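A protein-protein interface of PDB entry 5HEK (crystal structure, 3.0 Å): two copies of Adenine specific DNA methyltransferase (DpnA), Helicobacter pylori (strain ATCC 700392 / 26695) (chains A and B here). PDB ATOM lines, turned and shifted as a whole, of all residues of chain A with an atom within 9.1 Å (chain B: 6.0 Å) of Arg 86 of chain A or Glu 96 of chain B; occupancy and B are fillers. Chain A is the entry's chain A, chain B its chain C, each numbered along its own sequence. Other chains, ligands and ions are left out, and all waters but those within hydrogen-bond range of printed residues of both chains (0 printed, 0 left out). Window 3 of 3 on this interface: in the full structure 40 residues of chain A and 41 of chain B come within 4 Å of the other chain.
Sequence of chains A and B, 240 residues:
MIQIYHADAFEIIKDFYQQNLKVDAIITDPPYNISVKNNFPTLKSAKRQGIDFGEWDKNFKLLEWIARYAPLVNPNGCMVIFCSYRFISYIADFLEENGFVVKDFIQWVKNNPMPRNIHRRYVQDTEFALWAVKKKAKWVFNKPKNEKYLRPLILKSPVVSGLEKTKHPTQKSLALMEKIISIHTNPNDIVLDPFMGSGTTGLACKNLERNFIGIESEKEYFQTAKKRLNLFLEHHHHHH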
ATOM      1  N   TYR A  32     -22.406  -9.094 -11.877  1.00  0.00           N
ATOM      2  CA  TYR A  32     -22.740  -7.786 -12.468  1.00  0.00           C
ATOM      3  C   TYR A  32     -23.932  -7.863 -13.439  1.00  0.00           C
ATOM      4  O   TYR A  32     -25.073  -8.029 -13.006  1.00  0.00           O
ATOM      5  CB  TYR A  32     -21.534  -7.145 -13.163  1.00  0.00           C
ATOM      6  CG  TYR A  32     -21.715  -5.650 -13.371  1.00  0.00           C
ATOM      7  CD1 TYR A  32     -21.684  -4.768 -12.295  1.00  0.00           C
ATOM      8  CD2 TYR A  32     -21.945  -5.123 -14.641  1.00  0.00           C
ATOM      9  CE1 TYR A  32     -21.860  -3.403 -12.484  1.00  0.00           C
ATOM     10  CE2 TYR A  32     -22.126  -3.764 -14.836  1.00  0.00           C
ATOM     11  CZ  TYR A  32     -22.080  -2.911 -13.758  1.00  0.00           C
ATOM     12  OH  TYR A  32     -22.257  -1.563 -13.963  1.00  0.00           O
ATOM     13  N   ASN A  33     -23.655  -7.656 -14.729  1.00  0.00           N
ATOM     14  CA  ASN A  33     -24.649  -7.596 -15.822  1.00  0.00           C
ATOM     15  C   ASN A  33     -25.492  -6.321 -15.780  1.00  0.00           C
ATOM     16  O   ASN A  33     -25.209  -5.358 -16.500  1.00  0.00           O
ATOM     17  CB  ASN A  33     -25.578  -8.826 -15.831  1.00  0.00           C
ATOM     18  CG  ASN A  33     -24.878 -10.104 -16.290  1.00  0.00           C
ATOM     19  OD1 ASN A  33     -24.349 -10.861 -15.480  1.00  0.00           O
ATOM     20  ND2 ASN A  33     -24.889 -10.353 -17.595  1.00  0.00           N
ATOM     21  N   ASN A  59     -16.079  -3.310 -21.176  1.00  0.00           N
ATOM     22  CA  ASN A  59     -16.830  -4.532 -20.979  1.00  0.00           C
ATOM     23  C   ASN A  59     -15.968  -5.641 -21.560  1.00  0.00           C
ATOM     24  O   ASN A  59     -15.920  -5.826 -22.778  1.00  0.00           O
ATOM     25  CB  ASN A  59     -18.189  -4.456 -21.683  1.00  0.00           C
ATOM     26  CG  ASN A  59     -18.822  -3.081 -21.580  1.00  0.00           C
ATOM     27  OD1 ASN A  59     -18.730  -2.420 -20.547  1.00  0.00           O
ATOM     28  ND2 ASN A  59     -19.449  -2.633 -22.663  1.00  0.00           N
ATOM     29  N   CYS A  83     -29.332 -12.637 -18.056  1.00  0.00           N
ATOM     30  CA  CYS A  83     -28.761 -11.292 -18.109  1.00  0.00           C
ATOM     31  C   CYS A  83     -29.785 -10.142 -18.135  1.00  0.00           C
ATOM     32  O   CYS A  83     -31.011 -10.336 -18.088  1.00  0.00           O
ATOM     33  CB  CYS A  83     -27.827 -11.173 -19.310  1.00  0.00           C
ATOM     34  SG  CYS A  83     -28.576 -11.721 -20.831  1.00  0.00           S
ATOM     35  N   SER A  84     -29.240  -8.936 -18.236  1.00  0.00           N
ATOM     36  CA  SER A  84     -30.017  -7.714 -18.239  1.00  0.00           C
ATOM     37  C   SER A  84     -30.112  -7.163 -19.648  1.00  0.00           C
ATOM     38  O   SER A  84     -29.202  -7.356 -20.463  1.00  0.00           O
ATOM     39  CB  SER A  84     -29.376  -6.680 -17.315  1.00  0.00           C
ATOM     40  OG  SER A  84     -29.941  -5.396 -17.520  1.00  0.00           O
ATOM     41  N   TYR A  85     -31.222  -6.488 -19.936  1.00  0.00           N
ATOM     42  CA  TYR A  85     -31.448  -5.929 -21.263  1.00  0.00           C
ATOM     43  C   TYR A  85     -30.426  -4.851 -21.609  1.00  0.00           C
ATOM     44  O   TYR A  85     -30.313  -4.446 -22.773  1.00  0.00           O
ATOM     45  CB  TYR A  85     -32.867  -5.364 -21.373  1.00  0.00           C
ATOM     46  CG  TYR A  85     -33.089  -4.040 -20.678  1.00  0.00           C
ATOM     47  CD1 TYR A  85     -33.224  -3.973 -19.299  1.00  0.00           C
ATOM     48  CD2 TYR A  85     -33.200  -2.864 -21.407  1.00  0.00           C
ATOM     49  CE1 TYR A  85     -33.445  -2.774 -18.660  1.00  0.00           C
ATOM     50  CE2 TYR A  85     -33.424  -1.649 -20.779  1.00  0.00           C
ATOM     51  CZ  TYR A  85     -33.545  -1.613 -19.404  1.00  0.00           C
ATOM     52  OH  TYR A  85     -33.763  -0.413 -18.768  1.00  0.00           O
ATOM     53  N   ARG A  86     -29.670  -4.405 -20.606  1.00  0.00           N
ATOM     54  CA  ARG A  86     -28.625  -3.411 -20.825  1.00  0.00           C
ATOM     55  C   ARG A  86     -27.330  -4.065 -21.293  1.00  0.00           C
ATOM     56  O   ARG A  86     -26.349  -3.380 -21.582  1.00  0.00           O
ATOM     57  CB  ARG A  86     -28.370  -2.622 -19.545  1.00  0.00           C
ATOM     58  CG  ARG A  86     -29.614  -1.970 -19.001  1.00  0.00           C
ATOM     59  CD  ARG A  86     -30.157  -0.864 -19.921  1.00  0.00           C
ATOM     60  NE  ARG A  86     -29.512   0.430 -19.698  1.00  0.00           N
ATOM     61  CZ  ARG A  86     -28.487   0.888 -20.406  1.00  0.00           C
ATOM     62  NH1 ARG A  86     -27.977   0.158 -21.394  1.00  0.00           N
ATOM     63  NH2 ARG A  86     -27.964   2.073 -20.122  1.00  0.00           N
ATOM     64  N   PHE A  87     -27.346  -5.393 -21.382  1.00  0.00           N
ATOM     65  CA  PHE A  87     -26.152  -6.184 -21.669  1.00  0.00           C
ATOM     66  C   PHE A  87     -26.361  -7.166 -22.833  1.00  0.00           C
ATOM     67  O   PHE A  87     -25.471  -7.311 -23.669  1.00  0.00           O
ATOM     68  CB  PHE A  87     -25.622  -6.881 -20.417  1.00  0.00           C
ATOM     69  CG  PHE A  87     -24.117  -6.924 -20.376  1.00  0.00           C
ATOM     70  CD1 PHE A  87     -23.376  -5.766 -20.611  1.00  0.00           C
ATOM     71  CD2 PHE A  87     -23.441  -8.110 -20.121  1.00  0.00           C
ATOM     72  CE1 PHE A  87     -21.985  -5.794 -20.599  1.00  0.00           C
ATOM     73  CE2 PHE A  87     -22.050  -8.153 -20.099  1.00  0.00           C
ATOM     74  CZ  PHE A  87     -21.320  -6.988 -20.336  1.00  0.00           C
ATOM     75  N   ILE A  88     -27.486  -7.877 -22.857  1.00  0.00           N
ATOM     76  CA  ILE A  88     -27.709  -8.992 -23.797  1.00  0.00           C
ATOM     77  C   ILE A  88     -27.160  -8.800 -25.226  1.00  0.00           C
ATOM     78  O   ILE A  88     -26.701  -9.771 -25.836  1.00  0.00           O
ATOM     79  CB  ILE A  88     -29.230  -9.297 -23.971  1.00  0.00           C
ATOM     80  CG1 ILE A  88     -29.932  -8.166 -24.718  1.00  0.00           C
ATOM     81  CG2 ILE A  88     -29.928  -9.438 -22.656  1.00  0.00           C
ATOM     82  CD1 ILE A  88     -31.396  -8.381 -24.863  1.00  0.00           C
ATOM     83  N   SER A  89     -27.211  -7.582 -25.767  1.00  0.00           N
ATOM     84  CA  SER A  89     -26.666  -7.348 -27.101  1.00  0.00           C
ATOM     85  C   SER A  89     -25.166  -7.588 -27.115  1.00  0.00           C
ATOM     86  O   SER A  89     -24.631  -8.141 -28.083  1.00  0.00           O
ATOM     87  CB  SER A  89     -26.968  -5.925 -27.587  1.00  0.00           C
ATOM     88  OG  SER A  89     -28.358  -5.654 -27.620  1.00  0.00           O
ATOM     89  N   TYR A  90     -24.502  -7.147 -26.047  1.00  0.00           N
ATOM     90  CA  TYR A  90     -23.065  -7.338 -25.878  1.00  0.00           C
ATOM     91  C   TYR A  90     -22.713  -8.815 -25.709  1.00  0.00           C
ATOM     92  O   TYR A  90     -21.790  -9.327 -26.355  1.00  0.00           O
ATOM     93  CB  TYR A  90     -22.551  -6.520 -24.688  1.00  0.00           C
ATOM     94  CG  TYR A  90     -22.632  -5.017 -24.882  1.00  0.00           C
ATOM     95  CD1 TYR A  90     -23.779  -4.297 -24.547  1.00  0.00           C
ATOM     96  CD2 TYR A  90     -21.553  -4.318 -25.407  1.00  0.00           C
ATOM     97  CE1 TYR A  90     -23.840  -2.919 -24.729  1.00  0.00           C
ATOM     98  CE2 TYR A  90     -21.602  -2.948 -25.590  1.00  0.00           C
ATOM     99  CZ  TYR A  90     -22.744  -2.250 -25.255  1.00  0.00           C
ATOM    100  OH  TYR A  90     -22.770  -0.884 -25.454  1.00  0.00           O
ATOM    101  N   ILE A  91     -23.440  -9.491 -24.824  1.00  0.00           N
ATOM    102  CA  ILE A  91     -23.210 -10.907 -24.586  1.00  0.00           C
ATOM    103  C   ILE A  91     -23.407 -11.738 -25.860  1.00  0.00           C
ATOM    104  O   ILE A  91     -22.564 -12.575 -26.216  1.00  0.00           O
ATOM    105  CB  ILE A  91     -24.158 -11.433 -23.492  1.00  0.00           C
ATOM    106  CG1 ILE A  91     -23.846 -10.759 -22.161  1.00  0.00           C
ATOM    107  CG2 ILE A  91     -24.046 -12.944 -23.341  1.00  0.00           C
ATOM    108  CD1 ILE A  91     -24.770 -11.177 -21.057  1.00  0.00           C
ATOM    109  N   ARG A 121     -43.894   5.010 -13.325  1.00  0.00           N
ATOM    110  CA  ARG A 121     -43.063   4.029 -14.046  1.00  0.00           C
ATOM    111  C   ARG A 121     -43.674   2.619 -14.139  1.00  0.00           C
ATOM    112  O   ARG A 121     -44.600   2.283 -13.394  1.00  0.00           O
ATOM    113  CB  ARG A 121     -41.686   3.970 -13.364  1.00  0.00           C
ATOM    114  CG  ARG A 121     -40.563   3.320 -14.152  1.00  0.00           C
ATOM    115  CD  ARG A 121     -39.230   3.501 -13.423  1.00  0.00           C
ATOM    116  NE  ARG A 121     -38.112   2.836 -14.098  1.00  0.00           N
ATOM    117  CZ  ARG A 121     -36.831   3.028 -13.788  1.00  0.00           C
ATOM    118  NH1 ARG A 121     -36.493   3.884 -12.832  1.00  0.00           N
ATOM    119  NH2 ARG A 121     -35.883   2.381 -14.450  1.00  0.00           N
ATOM    120  N   PHE A 128     -34.653 -11.869 -18.047  1.00  0.00           N
ATOM    121  CA  PHE A 128     -34.289 -12.446 -19.343  1.00  0.00           C
ATOM    122  C   PHE A 128     -33.171 -13.454 -19.255  1.00  0.00           C
ATOM    123  O   PHE A 128     -32.368 -13.434 -18.322  1.00  0.00           O
ATOM    124  CB  PHE A 128     -33.858 -11.361 -20.318  1.00  0.00           C
ATOM    125  CG  PHE A 128     -34.966 -10.478 -20.758  1.00  0.00           C
ATOM    126  CD1 PHE A 128     -35.914 -10.929 -21.665  1.00  0.00           C
ATOM    127  CD2 PHE A 128     -35.053  -9.180 -20.275  1.00  0.00           C
ATOM    128  CE1 PHE A 128     -36.944 -10.100 -22.074  1.00  0.00           C
ATOM    129  CE2 PHE A 128     -36.071  -8.347 -20.677  1.00  0.00           C
ATOM    130  CZ  PHE A 128     -37.025  -8.802 -21.577  1.00  0.00           C
ATOM    131  N   ILE B  88     -31.020  -3.511 -28.551  1.00  0.00           N
ATOM    132  CA  ILE B  88     -31.604  -2.826 -27.405  1.00  0.00           C
ATOM    133  C   ILE B  88     -30.570  -2.410 -26.340  1.00  0.00           C
ATOM    134  O   ILE B  88     -30.699  -1.325 -25.759  1.00  0.00           O
ATOM    135  CB  ILE B  88     -32.693  -3.746 -26.763  1.00  0.00           C
ATOM    136  CG1 ILE B  88     -33.393  -3.085 -25.569  1.00  0.00           C
ATOM    137  CG2 ILE B  88     -32.096  -5.073 -26.332  1.00  0.00           C
ATOM    138  CD1 ILE B  88     -34.629  -3.863 -25.088  1.00  0.00           C
ATOM    139  N   SER B  89     -29.551  -3.235 -26.084  1.00  0.00           N
ATOM    140  CA  SER B  89     -28.484  -2.829 -25.156  1.00  0.00           C
ATOM    141  C   SER B  89     -27.644  -1.667 -25.685  1.00  0.00           C
ATOM    142  O   SER B  89     -27.205  -0.816 -24.909  1.00  0.00           O
ATOM    143  CB  SER B  89     -27.566  -3.998 -24.826  1.00  0.00           C
ATOM    144  OG  SER B  89     -28.306  -5.059 -24.256  1.00  0.00           O
ATOM    145  N   TYR B  90     -27.366  -1.675 -26.989  1.00  0.00           N
ATOM    146  CA  TYR B  90     -26.609  -0.601 -27.631  1.00  0.00           C
ATOM    147  C   TYR B  90     -27.392   0.709 -27.648  1.00  0.00           C
ATOM    148  O   TYR B  90     -26.913   1.748 -27.172  1.00  0.00           O
ATOM    149  CB  TYR B  90     -26.239  -0.997 -29.062  1.00  0.00           C
ATOM    150  CG  TYR B  90     -25.325  -2.207 -29.137  1.00  0.00           C
ATOM    151  CD1 TYR B  90     -24.086  -2.206 -28.508  1.00  0.00           C
ATOM    152  CD2 TYR B  90     -25.705  -3.353 -29.837  1.00  0.00           C
ATOM    153  CE1 TYR B  90     -23.259  -3.304 -28.570  1.00  0.00           C
ATOM    154  CE2 TYR B  90     -24.879  -4.460 -29.908  1.00  0.00           C
ATOM    155  CZ  TYR B  90     -23.653  -4.431 -29.271  1.00  0.00           C
ATOM    156  OH  TYR B  90     -22.802  -5.519 -29.321  1.00  0.00           O
ATOM    157  N   ILE B  91     -28.627   0.624 -28.139  1.00  0.00           N
ATOM    158  CA  ILE B  91     -29.504   1.780 -28.267  1.00  0.00           C
ATOM    159  C   ILE B  91     -29.664   2.448 -26.913  1.00  0.00           C
ATOM    160  O   ILE B  91     -29.680   3.674 -26.814  1.00  0.00           O
ATOM    161  CB  ILE B  91     -30.883   1.377 -28.838  1.00  0.00           C
ATOM    162  CG1 ILE B  91     -30.724   0.855 -30.269  1.00  0.00           C
ATOM    163  CG2 ILE B  91     -31.870   2.549 -28.810  1.00  0.00           C
ATOM    164  CD1 ILE B  91     -32.033   0.384 -30.896  1.00  0.00           C
ATOM    165  N   ALA B  92     -29.792   1.640 -25.871  1.00  0.00           N
ATOM    166  CA  ALA B  92     -29.936   2.179 -24.527  1.00  0.00           C
ATOM    167  C   ALA B  92     -28.704   2.991 -24.134  1.00  0.00           C
ATOM    168  O   ALA B  92     -28.823   4.116 -23.650  1.00  0.00           O
ATOM    169  CB  ALA B  92     -30.176   1.057 -23.528  1.00  0.00           C
ATOM    170  N   ASP B  93     -27.526   2.401 -24.315  1.00  0.00           N
ATOM    171  CA  ASP B  93     -26.270   3.077 -24.005  1.00  0.00           C
ATOM    172  C   ASP B  93     -26.064   4.327 -24.847  1.00  0.00           C
ATOM    173  O   ASP B  93     -25.628   5.356 -24.334  1.00  0.00           O
ATOM    174  CB  ASP B  93     -25.086   2.124 -24.190  1.00  0.00           C
ATOM    175  CG  ASP B  93     -24.962   1.130 -23.064  1.00  0.00           C
ATOM    176  OD1 ASP B  93     -25.357   1.468 -21.932  1.00  0.00           O
ATOM    177  OD2 ASP B  93     -24.489   0.007 -23.315  1.00  0.00           O
ATOM    178  N   PHE B  94     -26.394   4.240 -26.133  1.00  0.00           N
ATOM    179  CA  PHE B  94     -26.234   5.382 -27.031  1.00  0.00           C
ATOM    180  C   PHE B  94     -27.132   6.532 -26.583  1.00  0.00           C
ATOM    181  O   PHE B  94     -26.730   7.693 -26.624  1.00  0.00           O
ATOM    182  CB  PHE B  94     -26.568   5.000 -28.471  1.00  0.00           C
ATOM    183  CG  PHE B  94     -26.024   5.961 -29.492  1.00  0.00           C
ATOM    184  CD1 PHE B  94     -24.725   5.817 -29.984  1.00  0.00           C
ATOM    185  CD2 PHE B  94     -26.791   7.034 -29.933  1.00  0.00           C
ATOM    186  CE1 PHE B  94     -24.208   6.710 -30.922  1.00  0.00           C
ATOM    187  CE2 PHE B  94     -26.282   7.939 -30.865  1.00  0.00           C
ATOM    188  CZ  PHE B  94     -24.990   7.776 -31.365  1.00  0.00           C
ATOM    189  N   LEU B  95     -28.353   6.200 -26.172  1.00  0.00           N
ATOM    190  CA  LEU B  95     -29.290   7.184 -25.639  1.00  0.00           C
ATOM    191  C   LEU B  95     -28.733   7.921 -24.412  1.00  0.00           C
ATOM    192  O   LEU B  95     -28.862   9.140 -24.302  1.00  0.00           O
ATOM    193  CB  LEU B  95     -30.625   6.516 -25.285  1.00  0.00           C
ATOM    194  CG  LEU B  95     -31.577   6.175 -26.439  1.00  0.00           C
ATOM    195  CD1 LEU B  95     -32.749   5.353 -25.946  1.00  0.00           C
ATOM    196  CD2 LEU B  95     -32.074   7.424 -27.148  1.00  0.00           C
ATOM    197  N   GLU B  96     -28.122   7.182 -23.491  1.00  0.00           N
ATOM    198  CA  GLU B  96     -27.635   7.769 -22.242  1.00  0.00           C
ATOM    199  C   GLU B  96     -26.392   8.627 -22.470  1.00  0.00           C
ATOM    200  O   GLU B  96     -25.986   9.390 -21.591  1.00  0.00           O
ATOM    201  CB  GLU B  96     -27.348   6.673 -21.207  1.00  0.00           C
ATOM    202  CG  GLU B  96     -28.597   6.022 -20.614  1.00  0.00           C
ATOM    203  CD  GLU B  96     -28.289   5.154 -19.403  1.00  0.00           C
ATOM    204  OE1 GLU B  96     -27.103   4.796 -19.209  1.00  0.00           O
ATOM    205  OE2 GLU B  96     -29.235   4.833 -18.644  1.00  0.00           O
ATOM    206  N   GLU B  97     -25.805   8.504 -23.657  1.00  0.00           N
ATOM    207  CA  GLU B  97     -24.674   9.332 -24.056  1.00  0.00           C
ATOM    208  C   GLU B  97     -25.159  10.699 -24.589  1.00  0.00           C
ATOM    209  O   GLU B  97     -24.445  11.713 -24.540  1.00  0.00           O
ATOM    210  CB  GLU B  97     -23.857   8.581 -25.128  1.00  0.00           C
ATOM    211  CG  GLU B  97     -22.868   9.417 -25.952  1.00  0.00           C
ATOM    212  CD  GLU B  97     -21.808   8.571 -26.663  1.00  0.00           C
ATOM    213  OE1 GLU B  97     -21.827   7.330 -26.508  1.00  0.00           O
ATOM    214  OE2 GLU B  97     -20.956   9.148 -27.378  1.00  0.00           O
ATOM    215  N   ASN B  98     -26.399  10.713 -25.072  1.00  0.00           N
ATOM    216  CA  ASN B  98     -26.970  11.881 -25.724  1.00  0.00           C
ATOM    217  C   ASN B  98     -27.889  12.744 -24.857  1.00  0.00           C
ATOM    218  O   ASN B  98     -28.556  13.644 -25.370  1.00  0.00           O
ATOM    219  CB  ASN B  98     -27.693  11.446 -26.994  1.00  0.00           C
ATOM    220  CG  ASN B  98     -26.721  11.207 -28.147  1.00  0.00           C
ATOM    221  OD1 ASN B  98     -26.418  12.108 -28.916  1.00  0.00           O
ATOM    222  ND2 ASN B  98     -26.252   9.972 -28.277  1.00  0.00           N
ATOM    223  N   GLY B  99     -27.970  12.456 -23.563  1.00  0.00           N
ATOM    224  CA  GLY B  99     -28.752  13.301 -22.671  1.00  0.00           C
ATOM    225  C   GLY B  99     -30.110  12.734 -22.320  1.00  0.00           C
ATOM    226  O   GLY B  99     -31.001  13.442 -21.835  1.00  0.00           O
ATOM    227  N   PHE B 100     -30.266  11.440 -22.556  1.00  0.00           N
ATOM    228  CA  PHE B 100     -31.483  10.761 -22.172  1.00  0.00           C
ATOM    229  C   PHE B 100     -31.203   9.753 -21.068  1.00  0.00           C
ATOM    230  O   PHE B 100     -30.079   9.273 -20.923  1.00  0.00           O
ATOM    231  CB  PHE B 100     -32.093  10.065 -23.382  1.00  0.00           C
ATOM    232  CG  PHE B 100     -32.787  10.997 -24.314  1.00  0.00           C
ATOM    233  CD1 PHE B 100     -32.060  11.815 -25.171  1.00  0.00           C
ATOM    234  CD2 PHE B 100     -34.171  11.089 -24.305  1.00  0.00           C
ATOM    235  CE1 PHE B 100     -32.707  12.689 -26.028  1.00  0.00           C
ATOM    236  CE2 PHE B 100     -34.827  11.960 -25.151  1.00  0.00           C
ATOM    237  CZ  PHE B 100     -34.096  12.763 -26.015  1.00  0.00           C
ATOM    238  N   VAL B 101     -32.227   9.451 -20.278  1.00  0.00           N
ATOM    239  CA  VAL B 101     -32.134   8.401 -19.270  1.00  0.00           C
ATOM    240  C   VAL B 101     -33.040   7.241 -19.656  1.00  0.00           C
ATOM    241  O   VAL B 101     -34.255   7.426 -19.808  1.00  0.00           O
ATOM    242  CB  VAL B 101     -32.529   8.919 -17.873  1.00  0.00           C
ATOM    243  CG1 VAL B 101     -32.567   7.780 -16.853  1.00  0.00           C
ATOM    244  CG2 VAL B 101     -31.589  10.033 -17.439  1.00  0.00           C
ATOM    245  N   VAL B 102     -32.475   6.042 -19.792  1.00  0.00           N
ATOM    246  CA  VAL B 102     -33.311   4.916 -20.165  1.00  0.00           C
ATOM    247  C   VAL B 102     -34.051   4.505 -18.915  1.00  0.00           C
ATOM    248  O   VAL B 102     -33.452   4.046 -17.949  1.00  0.00           O
ATOM    249  CB  VAL B 102     -32.497   3.733 -20.698  1.00  0.00           C
ATOM    250  CG1 VAL B 102     -33.379   2.492 -20.819  1.00  0.00           C
ATOM    251  CG2 VAL B 102     -31.870   4.084 -22.028  1.00  0.00           C
ATOM    252  N   LYS B 135     -33.106  14.030 -19.616  1.00  0.00           N
ATOM    253  CA  LYS B 135     -32.411  13.781 -18.346  1.00  0.00           C
ATOM    254  C   LYS B 135     -33.110  14.358 -17.116  1.00  0.00           C
ATOM    255  O   LYS B 135     -33.480  13.612 -16.207  1.00  0.00           O
ATOM    256  CB  LYS B 135     -30.974  14.298 -18.411  1.00  0.00           C
ATOM    257  CG  LYS B 135     -29.964  13.165 -18.503  1.00  0.00           C
ATOM    258  CD  LYS B 135     -28.535  13.659 -18.638  1.00  0.00           C
ATOM    259  CE  LYS B 135     -27.543  12.499 -18.550  1.00  0.00           C
ATOM    260  NZ  LYS B 135     -26.614  12.444 -19.716  1.00  0.00           N
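Ile 88 of chain A touches Ser 89 of chain B, and with the chains exchanged Ser 89 of chain A touches Ile 88 of chain B. Ser 89 of chain B touches its own counterpart, Ser 89 of chain A. Ser 89 of chain A touches Tyr 90 of chain B, and with the chains exchanged Tyr 90 of chain A touches Ser 89 of chain B. Tyr 90 of chain B touches its own counterpart, Tyr 90 of chain A. Of the 15 pairs that touch across the chains among the printed residues, 7 have their exchanged pair printed and touching as well.
Among the printed residues, merely in contact across the chains: Arg 86 of chain A with Ala 92 of chain B, Arg 86 of chain A with Ser 89 of chain B, Tyr 90 of chain A with Tyr 90 of chain B, Ser 89 of chain A with Ile 88 of chain B, Tyr 85 of chain A with Val 102 of chain B, Ile 88 of chain A with Ile 88 of chain B and Tyr 90 of chain A with Ser 89 of chain B.
Of the 16 printed residues of chain B, 7 touch a printed residue of chain A. Printed residues of chain B that touch a printed residue of chain A: Ile 88, Ser 89, Tyr 90, Ala 92, Asp 93, Glu 96 and Val 102. Hydrophobic or aromatic side chains of chain B that line the printed part of chain A: Ile 88, Tyr 90, Ala 92 and Val 102. Along chain B the printed residues that touch a printed residue of chain A span positions 88 to 102. Hydrophobic or aromatic side chains of chain A that line the printed part of chain B: Tyr 85, Ile 88 and Tyr 90. Among the printed residues, Asp or Glu carboxylates within 4 Å of a Lys or Arg side-chain nitrogen of the other chain: Arg 86 of chain A with Asp 93 of chain B and Arg 86 of chain A with Glu 96 of chain B.
OG of Ser 84 of chain A lies close to N of Arg 86 of chain A (3.3 Å).
The side-chain carboxylate (OE1) of Glu 96 of chain B lies within salt-bridge range of the guanidinium group (NH2) of Arg 86 of chain A (3.0 Å). The guanidinium group (NH1) of Arg 86 of chain A is in salt-bridge range of the side-chain carboxylate (OD1) of Asp 93 of chain B. The backbone NH (N) of Ser 89 of chain B lies within hydrogen-bond range of the side-chain hydroxyl (OG) of Ser 89 of chain A, 3.1 Å away. The side-chain hydroxyl (OG) of Ser 89 of chain B is in hydrogen-bond range of the backbone NH (N) of Ile 88 of chain A (3.3 Å). The side-chain hydroxyl (OH) of Tyr 90 of chain B is in hydrogen-bond range of the backbone carbonyl oxygen (O) of Ser 89 of chain A (3.4 Å). The backbone carbonyl oxygen of Tyr 85 of chain A is in hydrogen-bond range of the side-chain hydroxyl of Ser 89 of chain B, 2.6 Å away. The backbone NH (N) of Phe 87 of chain A sits at hydrogen-bond distance from the side-chain hydroxyl (OG) of Ser 89 of chain B, at 3.0 Å. OH of Tyr 90 of chain A sits at hydrogen-bond distance from OD2 of Asp 93 of chain B (2.9 Å).
Asn 59 of chain A touches none of the printed residues of chain B. Arg 86 of chain A touches four residues of chain B. Of the printed residues of chain B, Ile 88 of chain A touches Ile 88 (3.7 Å) and Ser 89 (3.3 Å). Printed residues of chain B within 4 Å of Ser 89 of chain A: Ile 88, Ser 89 and Tyr 90. Printed residues of chain A within 4 Å of Ile 88 of chain B: Ile 88 and Ser 89. Of the printed residues of chain A, Ser 89 of chain B touches Tyr 85 (2.6 Å), Arg 86 (3.3 Å), Phe 87 (3.0 Å), Ile 88 (3.3 Å), Ser 89 (3.1 Å) and Tyr 90 (3.8 Å). Of the printed residues of chain A, Tyr 90 of chain B touches Ser 89 (3.4 Å) and Tyr 90 (3.4 Å). The nearest residue of chain A that does not touch Glu 96 of chain B is Tyr 85 of chain A (6.9 Å).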
